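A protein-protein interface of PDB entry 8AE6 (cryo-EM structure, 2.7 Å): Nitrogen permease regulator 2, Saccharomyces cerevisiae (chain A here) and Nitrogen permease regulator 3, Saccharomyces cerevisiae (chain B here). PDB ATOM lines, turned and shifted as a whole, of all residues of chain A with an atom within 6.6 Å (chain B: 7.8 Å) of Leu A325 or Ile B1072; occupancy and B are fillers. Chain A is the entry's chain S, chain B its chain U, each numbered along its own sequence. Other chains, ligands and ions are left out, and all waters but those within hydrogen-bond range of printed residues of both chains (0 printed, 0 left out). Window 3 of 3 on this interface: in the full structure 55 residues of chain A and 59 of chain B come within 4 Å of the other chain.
Ile A321 touches Ile B1143.
Arg A322 touches Leu B1074 (NH2 to CG, 3.4 Å).
O of Gly B1111 touches CD of Arg A322 (3.4 Å).
Leu A325 touches Asn B957.
Ile B1072 touches Leu A325.
Leu A325 touches Leu B1074.
OG1 of Thr A326 touches CD2 of Leu B1074, at 3.3 Å.
Phe A439 touches Ile B1141.
Phe A439 touches Ile B1143 (CZ to CD1, 3.9 Å).
CD1 of Ile B1141 touches OD1 of Asp A440, 3.8 Å away.
Of the printed residues of chain A, Ile B1072 touches Leu A325 and Phe A439.
Of the printed residues of chain B, Phe A439 touches Ile B1072 (3.98 Å), Ile B1141 (3.9 Å) and Ile B1143 (3.9 Å).
Printed residues of chain B within 4 Å of Ile A321: Ile B1143 (3.7 Å).
NH1 of Arg B959 lies within salt-bridge range of OD2 of Asp A440, at 2.6 Å.
The backbone carbonyl oxygen (O) of Asn B1110 lies within hydrogen-bond range of the guanidinium group (NE) of Arg A322.
OE1 of Glu B1075 sits at hydrogen-bond distance from ND2 of Asn B1110 (3.1 Å).
The backbone NH of Arg B959 sits at hydrogen-bond distance from the backbone carbonyl oxygen of Tyr B1139 (2.6 Å).
O of Phe B1109 lies close to OD1 of Asn B957 (3.5 Å).
The side-chain amide oxygen (OD1) of Asn B957 lies close to the backbone carbonyl oxygen (O) of Ile B1073, 3.1 Å away.
O of Asn B957 is in hydrogen-bond range of N of Ile B1141 (2.5 Å).
The guanidinium group (NH1) of Arg A322 is in hydrogen-bond range of the side-chain hydroxyl (OG1) of Thr A326.
Of the 22 printed residues of chain B, 8 touch a printed residue of chain A.
Hydrophobic or aromatic side chains of chain B that line the printed part of chain A: Ile B1072, Leu B1074, Ile B1141 and Ile B1143.
Along chain B the printed residues that touch a printed residue of chain A span positions 957 to 1143.
Of the 13 printed residues of chain A, 6 touch a printed residue of chain B.
Hydrophobic or aromatic side chains of chain A that line the printed part of chain B: Ile A321, Leu A325 and Phe A439.
Among the printed residues, Asp or Glu carboxylates within 4 Å of a Lys or Arg side-chain nitrogen of the other chain: Asp A440 with Arg B959.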
ATOM      1  N   ILE A 321     -29.570  20.777  23.570  1.00  0.00           N
ATOM      2  CA  ILE A 321     -29.255  19.979  24.749  1.00  0.00           C
ATOM      3  C   ILE A 321     -28.044  19.085  24.482  1.00  0.00           C
ATOM      4  O   ILE A 321     -27.318  18.716  25.411  1.00  0.00           O
ATOM      5  CB  ILE A 321     -30.509  19.188  25.184  1.00  0.00           C
ATOM      6  CG1 ILE A 321     -30.290  18.459  26.513  1.00  0.00           C
ATOM      7  CG2 ILE A 321     -30.952  18.229  24.095  1.00  0.00           C
ATOM      8  CD1 ILE A 321     -30.220  19.369  27.704  1.00  0.00           C
ATOM      9  N   ARG A 322     -27.781  18.765  23.216  1.00  0.00           N
ATOM     10  CA  ARG A 322     -26.590  18.011  22.847  1.00  0.00           C
ATOM     11  C   ARG A 322     -25.313  18.827  22.978  1.00  0.00           C
ATOM     12  O   ARG A 322     -24.224  18.245  22.957  1.00  0.00           O
ATOM     13  CB  ARG A 322     -26.728  17.490  21.420  1.00  0.00           C
ATOM     14  CG  ARG A 322     -26.060  16.155  21.178  1.00  0.00           C
ATOM     15  CD  ARG A 322     -26.271  15.707  19.752  1.00  0.00           C
ATOM     16  NE  ARG A 322     -25.274  14.736  19.326  1.00  0.00           N
ATOM     17  CZ  ARG A 322     -24.162  15.043  18.680  1.00  0.00           C
ATOM     18  NH1 ARG A 322     -23.854  16.296  18.395  1.00  0.00           N
ATOM     19  NH2 ARG A 322     -23.341  14.068  18.299  1.00  0.00           N
ATOM     20  N   ASN A 323     -25.413  20.151  23.112  1.00  0.00           N
ATOM     21  CA  ASN A 323     -24.241  20.977  23.371  1.00  0.00           C
ATOM     22  C   ASN A 323     -23.693  20.790  24.777  1.00  0.00           C
ATOM     23  O   ASN A 323     -22.579  21.242  25.051  1.00  0.00           O
ATOM     24  CB  ASN A 323     -24.568  22.451  23.140  1.00  0.00           C
ATOM     25  CG  ASN A 323     -24.734  22.785  21.676  1.00  0.00           C
ATOM     26  OD1 ASN A 323     -24.825  21.896  20.833  1.00  0.00           O
ATOM     27  ND2 ASN A 323     -24.773  24.077  21.366  1.00  0.00           N
ATOM     28  N   PHE A 324     -24.445  20.153  25.674  1.00  0.00           N
ATOM     29  CA  PHE A 324     -23.873  19.699  26.936  1.00  0.00           C
ATOM     30  C   PHE A 324     -22.867  18.581  26.711  1.00  0.00           C
ATOM     31  O   PHE A 324     -21.963  18.380  27.530  1.00  0.00           O
ATOM     32  CB  PHE A 324     -24.983  19.235  27.873  1.00  0.00           C
ATOM     33  CG  PHE A 324     -24.610  19.272  29.322  1.00  0.00           C
ATOM     34  CD1 PHE A 324     -24.704  20.443  30.044  1.00  0.00           C
ATOM     35  CD2 PHE A 324     -24.171  18.129  29.963  1.00  0.00           C
ATOM     36  CE1 PHE A 324     -24.366  20.475  31.377  1.00  0.00           C
ATOM     37  CE2 PHE A 324     -23.834  18.156  31.295  1.00  0.00           C
ATOM     38  CZ  PHE A 324     -23.930  19.331  32.003  1.00  0.00           C
ATOM     39  N   LEU A 325     -23.010  17.851  25.610  1.00  0.00           N
ATOM     40  CA  LEU A 325     -22.117  16.765  25.246  1.00  0.00           C
ATOM     41  C   LEU A 325     -20.996  17.226  24.325  1.00  0.00           C
ATOM     42  O   LEU A 325     -19.833  16.869  24.542  1.00  0.00           O
ATOM     43  CB  LEU A 325     -22.924  15.655  24.570  1.00  0.00           C
ATOM     44  CG  LEU A 325     -23.947  14.965  25.465  1.00  0.00           C
ATOM     45  CD1 LEU A 325     -24.801  14.009  24.673  1.00  0.00           C
ATOM     46  CD2 LEU A 325     -23.227  14.223  26.553  1.00  0.00           C
ATOM     47  N   THR A 326     -21.321  18.012  23.301  1.00  0.00           N
ATOM     48  CA  THR A 326     -20.338  18.441  22.309  1.00  0.00           C
ATOM     49  C   THR A 326     -19.827  19.837  22.664  1.00  0.00           C
ATOM     50  O   THR A 326     -20.053  20.826  21.965  1.00  0.00           O
ATOM     51  CB  THR A 326     -20.952  18.396  20.909  1.00  0.00           C
ATOM     52  OG1 THR A 326     -21.676  17.172  20.751  1.00  0.00           O
ATOM     53  CG2 THR A 326     -19.860  18.431  19.842  1.00  0.00           C
ATOM     54  N   ASP A 327     -19.140  19.902  23.803  1.00  0.00           N
ATOM     55  CA  ASP A 327     -18.485  21.116  24.272  1.00  0.00           C
ATOM     56  C   ASP A 327     -17.437  20.743  25.310  1.00  0.00           C
ATOM     57  O   ASP A 327     -17.744  20.024  26.270  1.00  0.00           O
ATOM     58  CB  ASP A 327     -19.492  22.102  24.866  1.00  0.00           C
ATOM     59  CG  ASP A 327     -18.931  23.500  24.996  1.00  0.00           C
ATOM     60  OD1 ASP A 327     -18.894  24.222  23.979  1.00  0.00           O
ATOM     61  OD2 ASP A 327     -18.528  23.878  26.115  1.00  0.00           O
ATOM     62  N   PRO A 328     -16.193  21.207  25.160  1.00  0.00           N
ATOM     63  CA  PRO A 328     -15.135  20.785  26.084  1.00  0.00           C
ATOM     64  C   PRO A 328     -15.179  21.456  27.445  1.00  0.00           C
ATOM     65  O   PRO A 328     -14.504  20.978  28.366  1.00  0.00           O
ATOM     66  CB  PRO A 328     -13.853  21.164  25.333  1.00  0.00           C
ATOM     67  CG  PRO A 328     -14.256  22.327  24.496  1.00  0.00           C
ATOM     68  CD  PRO A 328     -15.683  22.086  24.094  1.00  0.00           C
ATOM     69  N   MET A 330     -18.353  22.975  28.912  1.00  0.00           N
ATOM     70  CA  MET A 330     -19.678  23.224  29.470  1.00  0.00           C
ATOM     71  C   MET A 330     -19.945  22.368  30.702  1.00  0.00           C
ATOM     72  O   MET A 330     -20.447  22.869  31.712  1.00  0.00           O
ATOM     73  CB  MET A 330     -20.755  22.977  28.412  1.00  0.00           C
ATOM     74  CG  MET A 330     -22.136  23.474  28.813  1.00  0.00           C
ATOM     75  SD  MET A 330     -23.348  23.349  27.486  1.00  0.00           S
ATOM     76  CE  MET A 330     -22.691  24.532  26.313  1.00  0.00           C
ATOM     77  N   ALA A 331     -19.605  21.080  30.637  1.00  0.00           N
ATOM     78  CA  ALA A 331     -19.918  20.173  31.736  1.00  0.00           C
ATOM     79  C   ALA A 331     -19.036  20.433  32.953  1.00  0.00           C
ATOM     80  O   ALA A 331     -19.504  20.333  34.093  1.00  0.00           O
ATOM     81  CB  ALA A 331     -19.785  18.726  31.267  1.00  0.00           C
ATOM     82  N   SER A 436     -22.526  13.086  33.998  1.00  0.00           N
ATOM     83  CA  SER A 436     -23.649  12.235  33.622  1.00  0.00           C
ATOM     84  C   SER A 436     -24.873  12.530  34.476  1.00  0.00           C
ATOM     85  O   SER A 436     -26.001  12.531  33.971  1.00  0.00           O
ATOM     86  CB  SER A 436     -23.249  10.768  33.743  1.00  0.00           C
ATOM     87  OG  SER A 436     -22.165  10.471  32.880  1.00  0.00           O
ATOM     88  N   PHE A 439     -26.333  15.815  33.163  1.00  0.00           N
ATOM     89  CA  PHE A 439     -27.040  15.611  31.902  1.00  0.00           C
ATOM     90  C   PHE A 439     -28.361  14.886  32.114  1.00  0.00           C
ATOM     91  O   PHE A 439     -29.372  15.244  31.499  1.00  0.00           O
ATOM     92  CB  PHE A 439     -26.159  14.845  30.919  1.00  0.00           C
ATOM     93  CG  PHE A 439     -26.696  14.827  29.521  1.00  0.00           C
ATOM     94  CD1 PHE A 439     -26.881  16.007  28.825  1.00  0.00           C
ATOM     95  CD2 PHE A 439     -27.025  13.636  28.906  1.00  0.00           C
ATOM     96  CE1 PHE A 439     -27.378  15.996  27.541  1.00  0.00           C
ATOM     97  CE2 PHE A 439     -27.523  13.619  27.622  1.00  0.00           C
ATOM     98  CZ  PHE A 439     -27.700  14.802  26.940  1.00  0.00           C
ATOM     99  N   ASP A 440     -28.378  13.877  32.991  1.00  0.00           N
ATOM    100  CA  ASP A 440     -29.614  13.154  33.275  1.00  0.00           C
ATOM    101  C   ASP A 440     -30.630  14.037  33.984  1.00  0.00           C
ATOM    102  O   ASP A 440     -31.840  13.849  33.811  1.00  0.00           O
ATOM    103  CB  ASP A 440     -29.317  11.915  34.114  1.00  0.00           C
ATOM    104  CG  ASP A 440     -28.551  10.865  33.345  1.00  0.00           C
ATOM    105  OD1 ASP A 440     -28.116  11.157  32.212  1.00  0.00           O
ATOM    106  OD2 ASP A 440     -28.382   9.745  33.871  1.00  0.00           O
ATOM    107  N   ASN B 957     -29.456   8.583  22.467  1.00  0.00           N
ATOM    108  CA  ASN B 957     -28.015   8.457  22.594  1.00  0.00           C
ATOM    109  C   ASN B 957     -27.711   7.229  23.440  1.00  0.00           C
ATOM    110  O   ASN B 957     -28.531   6.807  24.259  1.00  0.00           O
ATOM    111  CB  ASN B 957     -27.399   9.714  23.204  1.00  0.00           C
ATOM    112  CG  ASN B 957     -26.031  10.020  22.644  1.00  0.00           C
ATOM    113  OD1 ASN B 957     -25.425   9.188  21.967  1.00  0.00           O
ATOM    114  ND2 ASN B 957     -25.541  11.223  22.903  1.00  0.00           N
ATOM    115  N   ILE B 958     -26.540   6.641  23.224  1.00  0.00           N
ATOM    116  CA  ILE B 958     -26.192   5.356  23.822  1.00  0.00           C
ATOM    117  C   ILE B 958     -25.191   5.580  24.947  1.00  0.00           C
ATOM    118  O   ILE B 958     -24.264   6.393  24.826  1.00  0.00           O
ATOM    119  CB  ILE B 958     -25.663   4.381  22.749  1.00  0.00           C
ATOM    120  CG1 ILE B 958     -25.311   3.024  23.357  1.00  0.00           C
ATOM    121  CG2 ILE B 958     -24.506   4.986  21.955  1.00  0.00           C
ATOM    122  CD1 ILE B 958     -26.513   2.223  23.790  1.00  0.00           C
ATOM    123  N   ARG B 959     -25.402   4.889  26.065  1.00  0.00           N
ATOM    124  CA  ARG B 959     -24.639   5.092  27.287  1.00  0.00           C
ATOM    125  C   ARG B 959     -24.156   3.750  27.816  1.00  0.00           C
ATOM    126  O   ARG B 959     -24.884   2.754  27.757  1.00  0.00           O
ATOM    127  CB  ARG B 959     -25.495   5.804  28.328  1.00  0.00           C
ATOM    128  CG  ARG B 959     -24.763   6.281  29.545  1.00  0.00           C
ATOM    129  CD  ARG B 959     -25.696   7.103  30.400  1.00  0.00           C
ATOM    130  NE  ARG B 959     -26.853   6.321  30.818  1.00  0.00           N
ATOM    131  CZ  ARG B 959     -27.857   6.798  31.537  1.00  0.00           C
ATOM    132  NH1 ARG B 959     -27.868   8.050  31.960  1.00  0.00           N
ATOM    133  NH2 ARG B 959     -28.873   5.998  31.843  1.00  0.00           N
ATOM    134  N   VAL B 960     -22.929   3.723  28.329  1.00  0.00           N
ATOM    135  CA  VAL B 960     -22.277   2.491  28.760  1.00  0.00           C
ATOM    136  C   VAL B 960     -21.786   2.664  30.193  1.00  0.00           C
ATOM    137  O   VAL B 960     -21.095   3.638  30.509  1.00  0.00           O
ATOM    138  CB  VAL B 960     -21.119   2.119  27.810  1.00  0.00           C
ATOM    139  CG1 VAL B 960     -20.164   1.129  28.460  1.00  0.00           C
ATOM    140  CG2 VAL B 960     -21.670   1.555  26.521  1.00  0.00           C
ATOM    141  N   ASP B 961     -22.148   1.714  31.059  1.00  0.00           N
ATOM    142  CA  ASP B 961     -21.796   1.738  32.470  1.00  0.00           C
ATOM    143  C   ASP B 961     -20.526   0.922  32.722  1.00  0.00           C
ATOM    144  O   ASP B 961     -19.831   0.503  31.791  1.00  0.00           O
ATOM    145  CB  ASP B 961     -22.971   1.235  33.313  1.00  0.00           C
ATOM    146  CG  ASP B 961     -23.522  -0.090  32.825  1.00  0.00           C
ATOM    147  OD1 ASP B 961     -23.051  -0.590  31.783  1.00  0.00           O
ATOM    148  OD2 ASP B 961     -24.432  -0.635  33.484  1.00  0.00           O
ATOM    149  N   LYS B 965     -17.979  -2.205  30.557  1.00  0.00           N
ATOM    150  CA  LYS B 965     -16.538  -1.993  30.469  1.00  0.00           C
ATOM    151  C   LYS B 965     -15.763  -3.161  31.068  1.00  0.00           C
ATOM    152  O   LYS B 965     -14.763  -3.611  30.497  1.00  0.00           O
ATOM    153  CB  LYS B 965     -16.158  -0.688  31.165  1.00  0.00           C
ATOM    154  CG  LYS B 965     -16.561   0.566  30.407  1.00  0.00           C
ATOM    155  CD  LYS B 965     -16.210   1.816  31.196  1.00  0.00           C
ATOM    156  CE  LYS B 965     -16.713   3.069  30.501  1.00  0.00           C
ATOM    157  NZ  LYS B 965     -16.461   4.293  31.308  1.00  0.00           N
ATOM    158  N   ASP B1069     -19.261   3.992  36.610  1.00  0.00           N
ATOM    159  CA  ASP B1069     -18.342   4.692  35.713  1.00  0.00           C
ATOM    160  C   ASP B1069     -18.938   4.717  34.294  1.00  0.00           C
ATOM    161  O   ASP B1069     -18.666   3.824  33.491  1.00  0.00           O
ATOM    162  CB  ASP B1069     -16.975   4.017  35.707  1.00  0.00           C
ATOM    163  CG  ASP B1069     -16.405   3.842  37.101  1.00  0.00           C
ATOM    164  OD1 ASP B1069     -17.005   4.363  38.065  1.00  0.00           O
ATOM    165  OD2 ASP B1069     -15.354   3.182  37.233  1.00  0.00           O
ATOM    166  N   TYR B1070     -19.759   5.727  33.991  1.00  0.00           N
ATOM    167  CA  TYR B1070     -20.537   5.761  32.736  1.00  0.00           C
ATOM    168  C   TYR B1070     -19.794   6.405  31.565  1.00  0.00           C
ATOM    169  O   TYR B1070     -18.677   6.887  31.751  1.00  0.00           O
ATOM    170  CB  TYR B1070     -21.884   6.458  32.954  1.00  0.00           C
ATOM    171  CG  TYR B1070     -23.019   5.494  33.209  1.00  0.00           C
ATOM    172  CD1 TYR B1070     -23.449   5.219  34.499  1.00  0.00           C
ATOM    173  CD2 TYR B1070     -23.653   4.851  32.157  1.00  0.00           C
ATOM    174  CE1 TYR B1070     -24.488   4.336  34.731  1.00  0.00           C
ATOM    175  CE2 TYR B1070     -24.692   3.970  32.378  1.00  0.00           C
ATOM    176  CZ  TYR B1070     -25.106   3.715  33.666  1.00  0.00           C
ATOM    177  OH  TYR B1070     -26.138   2.834  33.891  1.00  0.00           O
ATOM    178  N   THR B1071     -20.407   6.448  30.375  1.00  0.00           N
ATOM    179  CA  THR B1071     -19.699   6.944  29.202  1.00  0.00           C
ATOM    180  C   THR B1071     -20.685   7.002  28.049  1.00  0.00           C
ATOM    181  O   THR B1071     -21.289   5.983  27.699  1.00  0.00           O
ATOM    182  CB  THR B1071     -18.506   6.051  28.854  1.00  0.00           C
ATOM    183  OG1 THR B1071     -17.470   6.242  29.824  1.00  0.00           O
ATOM    184  CG2 THR B1071     -17.964   6.388  27.477  1.00  0.00           C
ATOM    185  N   ILE B1072     -20.852   8.182  27.465  1.00  0.00           N
ATOM    186  CA  ILE B1072     -21.804   8.395  26.384  1.00  0.00           C
ATOM    187  C   ILE B1072     -21.038   8.346  25.072  1.00  0.00           C
ATOM    188  O   ILE B1072     -20.190   9.204  24.804  1.00  0.00           O
ATOM    189  CB  ILE B1072     -22.557   9.723  26.541  1.00  0.00           C
ATOM    190  CG1 ILE B1072     -23.422   9.694  27.799  1.00  0.00           C
ATOM    191  CG2 ILE B1072     -23.411   9.993  25.317  1.00  0.00           C
ATOM    192  CD1 ILE B1072     -24.245  10.933  28.000  1.00  0.00           C
ATOM    193  N   ILE B1073     -21.333   7.343  24.254  1.00  0.00           N
ATOM    194  CA  ILE B1073     -20.735   7.229  22.930  1.00  0.00           C
ATOM    195  C   ILE B1073     -21.506   8.159  22.002  1.00  0.00           C
ATOM    196  O   ILE B1073     -22.663   7.895  21.663  1.00  0.00           O
ATOM    197  CB  ILE B1073     -20.750   5.786  22.424  1.00  0.00           C
ATOM    198  CG1 ILE B1073     -19.976   4.894  23.392  1.00  0.00           C
ATOM    199  CG2 ILE B1073     -20.146   5.703  21.035  1.00  0.00           C
ATOM    200  CD1 ILE B1073     -20.038   3.429  23.059  1.00  0.00           C
ATOM    201  N   LEU B1074     -20.865   9.258  21.602  1.00  0.00           N
ATOM    202  CA  LEU B1074     -21.579  10.346  20.943  1.00  0.00           C
ATOM    203  C   LEU B1074     -21.995   9.977  19.525  1.00  0.00           C
ATOM    204  O   LEU B1074     -23.145  10.200  19.134  1.00  0.00           O
ATOM    205  CB  LEU B1074     -20.708  11.598  20.945  1.00  0.00           C
ATOM    206  CG  LEU B1074     -21.449  12.923  20.862  1.00  0.00           C
ATOM    207  CD1 LEU B1074     -22.466  13.012  21.972  1.00  0.00           C
ATOM    208  CD2 LEU B1074     -20.465  14.073  20.947  1.00  0.00           C
ATOM    209  N   GLU B1075     -21.079   9.412  18.742  1.00  0.00           N
ATOM    210  CA  GLU B1075     -21.367   8.983  17.376  1.00  0.00           C
ATOM    211  C   GLU B1075     -20.919   7.533  17.266  1.00  0.00           C
ATOM    212  O   GLU B1075     -19.733   7.255  17.043  1.00  0.00           O
ATOM    213  CB  GLU B1075     -20.666   9.868  16.350  1.00  0.00           C
ATOM    214  CG  GLU B1075     -21.043   9.564  14.910  1.00  0.00           C
ATOM    215  CD  GLU B1075     -22.435  10.041  14.557  1.00  0.00           C
ATOM    216  OE1 GLU B1075     -22.876  11.056  15.133  1.00  0.00           O
ATOM    217  OE2 GLU B1075     -23.088   9.401  13.705  1.00  0.00           O
ATOM    218  N   PRO B1076     -21.838   6.579  17.434  1.00  0.00           N
ATOM    219  CA  PRO B1076     -21.442   5.163  17.458  1.00  0.00           C
ATOM    220  C   PRO B1076     -21.007   4.606  16.111  1.00  0.00           C
ATOM    221  O   PRO B1076     -20.480   3.487  16.074  1.00  0.00           O
ATOM    222  CB  PRO B1076     -22.701   4.450  17.967  1.00  0.00           C
ATOM    223  CG  PRO B1076     -23.803   5.392  17.736  1.00  0.00           C
ATOM    224  CD  PRO B1076     -23.252   6.770  17.787  1.00  0.00           C
ATOM    225  N   GLU B1083     -14.852   0.903  22.041  1.00  0.00           N
ATOM    226  CA  GLU B1083     -16.203   1.438  22.160  1.00  0.00           C
ATOM    227  C   GLU B1083     -17.215   0.626  21.361  1.00  0.00           C
ATOM    228  O   GLU B1083     -18.372   0.506  21.774  1.00  0.00           O
ATOM    229  CB  GLU B1083     -16.222   2.899  21.726  1.00  0.00           C
ATOM    230  CG  GLU B1083     -15.538   3.820  22.706  1.00  0.00           C
ATOM    231  CD  GLU B1083     -14.725   4.887  22.019  1.00  0.00           C
ATOM    232  OE1 GLU B1083     -15.033   5.203  20.851  1.00  0.00           O
ATOM    233  OE2 GLU B1083     -13.781   5.414  22.644  1.00  0.00           O
ATOM    234  N   TRP B1086     -18.114  -2.005  23.491  1.00  0.00           N
ATOM    235  CA  TRP B1086     -19.083  -1.553  24.484  1.00  0.00           C
ATOM    236  C   TRP B1086     -20.502  -1.582  23.930  1.00  0.00           C
ATOM    237  O   TRP B1086     -21.447  -1.935  24.643  1.00  0.00           O
ATOM    238  CB  TRP B1086     -18.734  -0.141  24.960  1.00  0.00           C
ATOM    239  CG  TRP B1086     -17.486  -0.047  25.766  1.00  0.00           C
ATOM    240  CD1 TRP B1086     -16.798  -1.071  26.333  1.00  0.00           C
ATOM    241  CD2 TRP B1086     -16.773   1.148  26.103  1.00  0.00           C
ATOM    242  NE1 TRP B1086     -15.699  -0.594  27.002  1.00  0.00           N
ATOM    243  CE2 TRP B1086     -15.663   0.768  26.874  1.00  0.00           C
ATOM    244  CE3 TRP B1086     -16.968   2.503  25.826  1.00  0.00           C
ATOM    245  CZ2 TRP B1086     -14.749   1.690  27.371  1.00  0.00           C
ATOM    246  CZ3 TRP B1086     -16.061   3.418  26.321  1.00  0.00           C
ATOM    247  CH2 TRP B1086     -14.966   3.007  27.085  1.00  0.00           C
ATOM    248  N   PHE B1109     -28.227   6.476  16.537  1.00  0.00           N
ATOM    249  CA  PHE B1109     -28.280   6.722  17.977  1.00  0.00           C
ATOM    250  C   PHE B1109     -27.199   7.724  18.384  1.00  0.00           C
ATOM    251  O   PHE B1109     -26.267   7.416  19.123  1.00  0.00           O
ATOM    252  CB  PHE B1109     -28.134   5.414  18.746  1.00  0.00           C
ATOM    253  CG  PHE B1109     -29.359   4.538  18.721  1.00  0.00           C
ATOM    254  CD1 PHE B1109     -30.545   4.972  18.153  1.00  0.00           C
ATOM    255  CD2 PHE B1109     -29.319   3.273  19.278  1.00  0.00           C
ATOM    256  CE1 PHE B1109     -31.658   4.161  18.138  1.00  0.00           C
ATOM    257  CE2 PHE B1109     -30.430   2.459  19.263  1.00  0.00           C
ATOM    258  CZ  PHE B1109     -31.600   2.905  18.693  1.00  0.00           C
ATOM    259  N   ASN B1110     -27.342   8.953  17.887  1.00  0.00           N
ATOM    260  CA  ASN B1110     -26.338   9.984  18.112  1.00  0.00           C
ATOM    261  C   ASN B1110     -26.916  11.287  18.652  1.00  0.00           C
ATOM    262  O   ASN B1110     -26.177  12.271  18.773  1.00  0.00           O
ATOM    263  CB  ASN B1110     -25.566  10.266  16.820  1.00  0.00           C
ATOM    264  CG  ASN B1110     -26.477  10.477  15.631  1.00  0.00           C
ATOM    265  OD1 ASN B1110     -27.698  10.440  15.756  1.00  0.00           O
ATOM    266  ND2 ASN B1110     -25.883  10.698  14.467  1.00  0.00           N
ATOM    267  N   GLY B1111     -28.202  11.325  18.981  1.00  0.00           N
ATOM    268  CA  GLY B1111     -28.795  12.552  19.473  1.00  0.00           C
ATOM    269  C   GLY B1111     -29.091  13.581  18.407  1.00  0.00           C
ATOM    270  O   GLY B1111     -29.372  14.734  18.738  1.00  0.00           O
ATOM    271  N   TYR B1139     -29.164   1.940  29.231  1.00  0.00           N
ATOM    272  CA  TYR B1139     -28.143   2.211  28.230  1.00  0.00           C
ATOM    273  C   TYR B1139     -28.549   3.269  27.217  1.00  0.00           C
ATOM    274  O   TYR B1139     -27.674   3.834  26.553  1.00  0.00           O
ATOM    275  CB  TYR B1139     -27.788   0.920  27.495  1.00  0.00           C
ATOM    276  CG  TYR B1139     -27.301  -0.186  28.399  1.00  0.00           C
ATOM    277  CD1 TYR B1139     -26.139  -0.039  29.142  1.00  0.00           C
ATOM    278  CD2 TYR B1139     -28.008  -1.373  28.519  1.00  0.00           C
ATOM    279  CE1 TYR B1139     -25.689  -1.047  29.970  1.00  0.00           C
ATOM    280  CE2 TYR B1139     -27.566  -2.388  29.345  1.00  0.00           C
ATOM    281  CZ  TYR B1139     -26.407  -2.218  30.068  1.00  0.00           C
ATOM    282  OH  TYR B1139     -25.964  -3.224  30.895  1.00  0.00           O
ATOM    283  N   ILE B1141     -30.125   6.899  26.227  1.00  0.00           N
ATOM    284  CA  ILE B1141     -30.448   8.258  26.628  1.00  0.00           C
ATOM    285  C   ILE B1141     -31.649   8.715  25.814  1.00  0.00           C
ATOM    286  O   ILE B1141     -31.667   8.579  24.588  1.00  0.00           O
ATOM    287  CB  ILE B1141     -29.231   9.177  26.408  1.00  0.00           C
ATOM    288  CG1 ILE B1141     -28.211   9.010  27.535  1.00  0.00           C
ATOM    289  CG2 ILE B1141     -29.637  10.623  26.202  1.00  0.00           C
ATOM    290  CD1 ILE B1141     -28.677   9.519  28.867  1.00  0.00           C
ATOM    291  N   ILE B1143     -33.834  11.813  24.598  1.00  0.00           N
ATOM    292  CA  ILE B1143     -33.767  13.253  24.389  1.00  0.00           C
ATOM    293  C   ILE B1143     -34.992  13.662  23.585  1.00  0.00           C
ATOM    294  O   ILE B1143     -35.244  13.112  22.507  1.00  0.00           O
ATOM    295  CB  ILE B1143     -32.470  13.661  23.673  1.00  0.00           C
ATOM    296  CG1 ILE B1143     -31.286  13.580  24.637  1.00  0.00           C
ATOM    297  CG2 ILE B1143     -32.584  15.054  23.091  1.00  0.00           C
ATOM    298  CD1 ILE B1143     -29.941  13.645  23.952  1.00  0.00           C
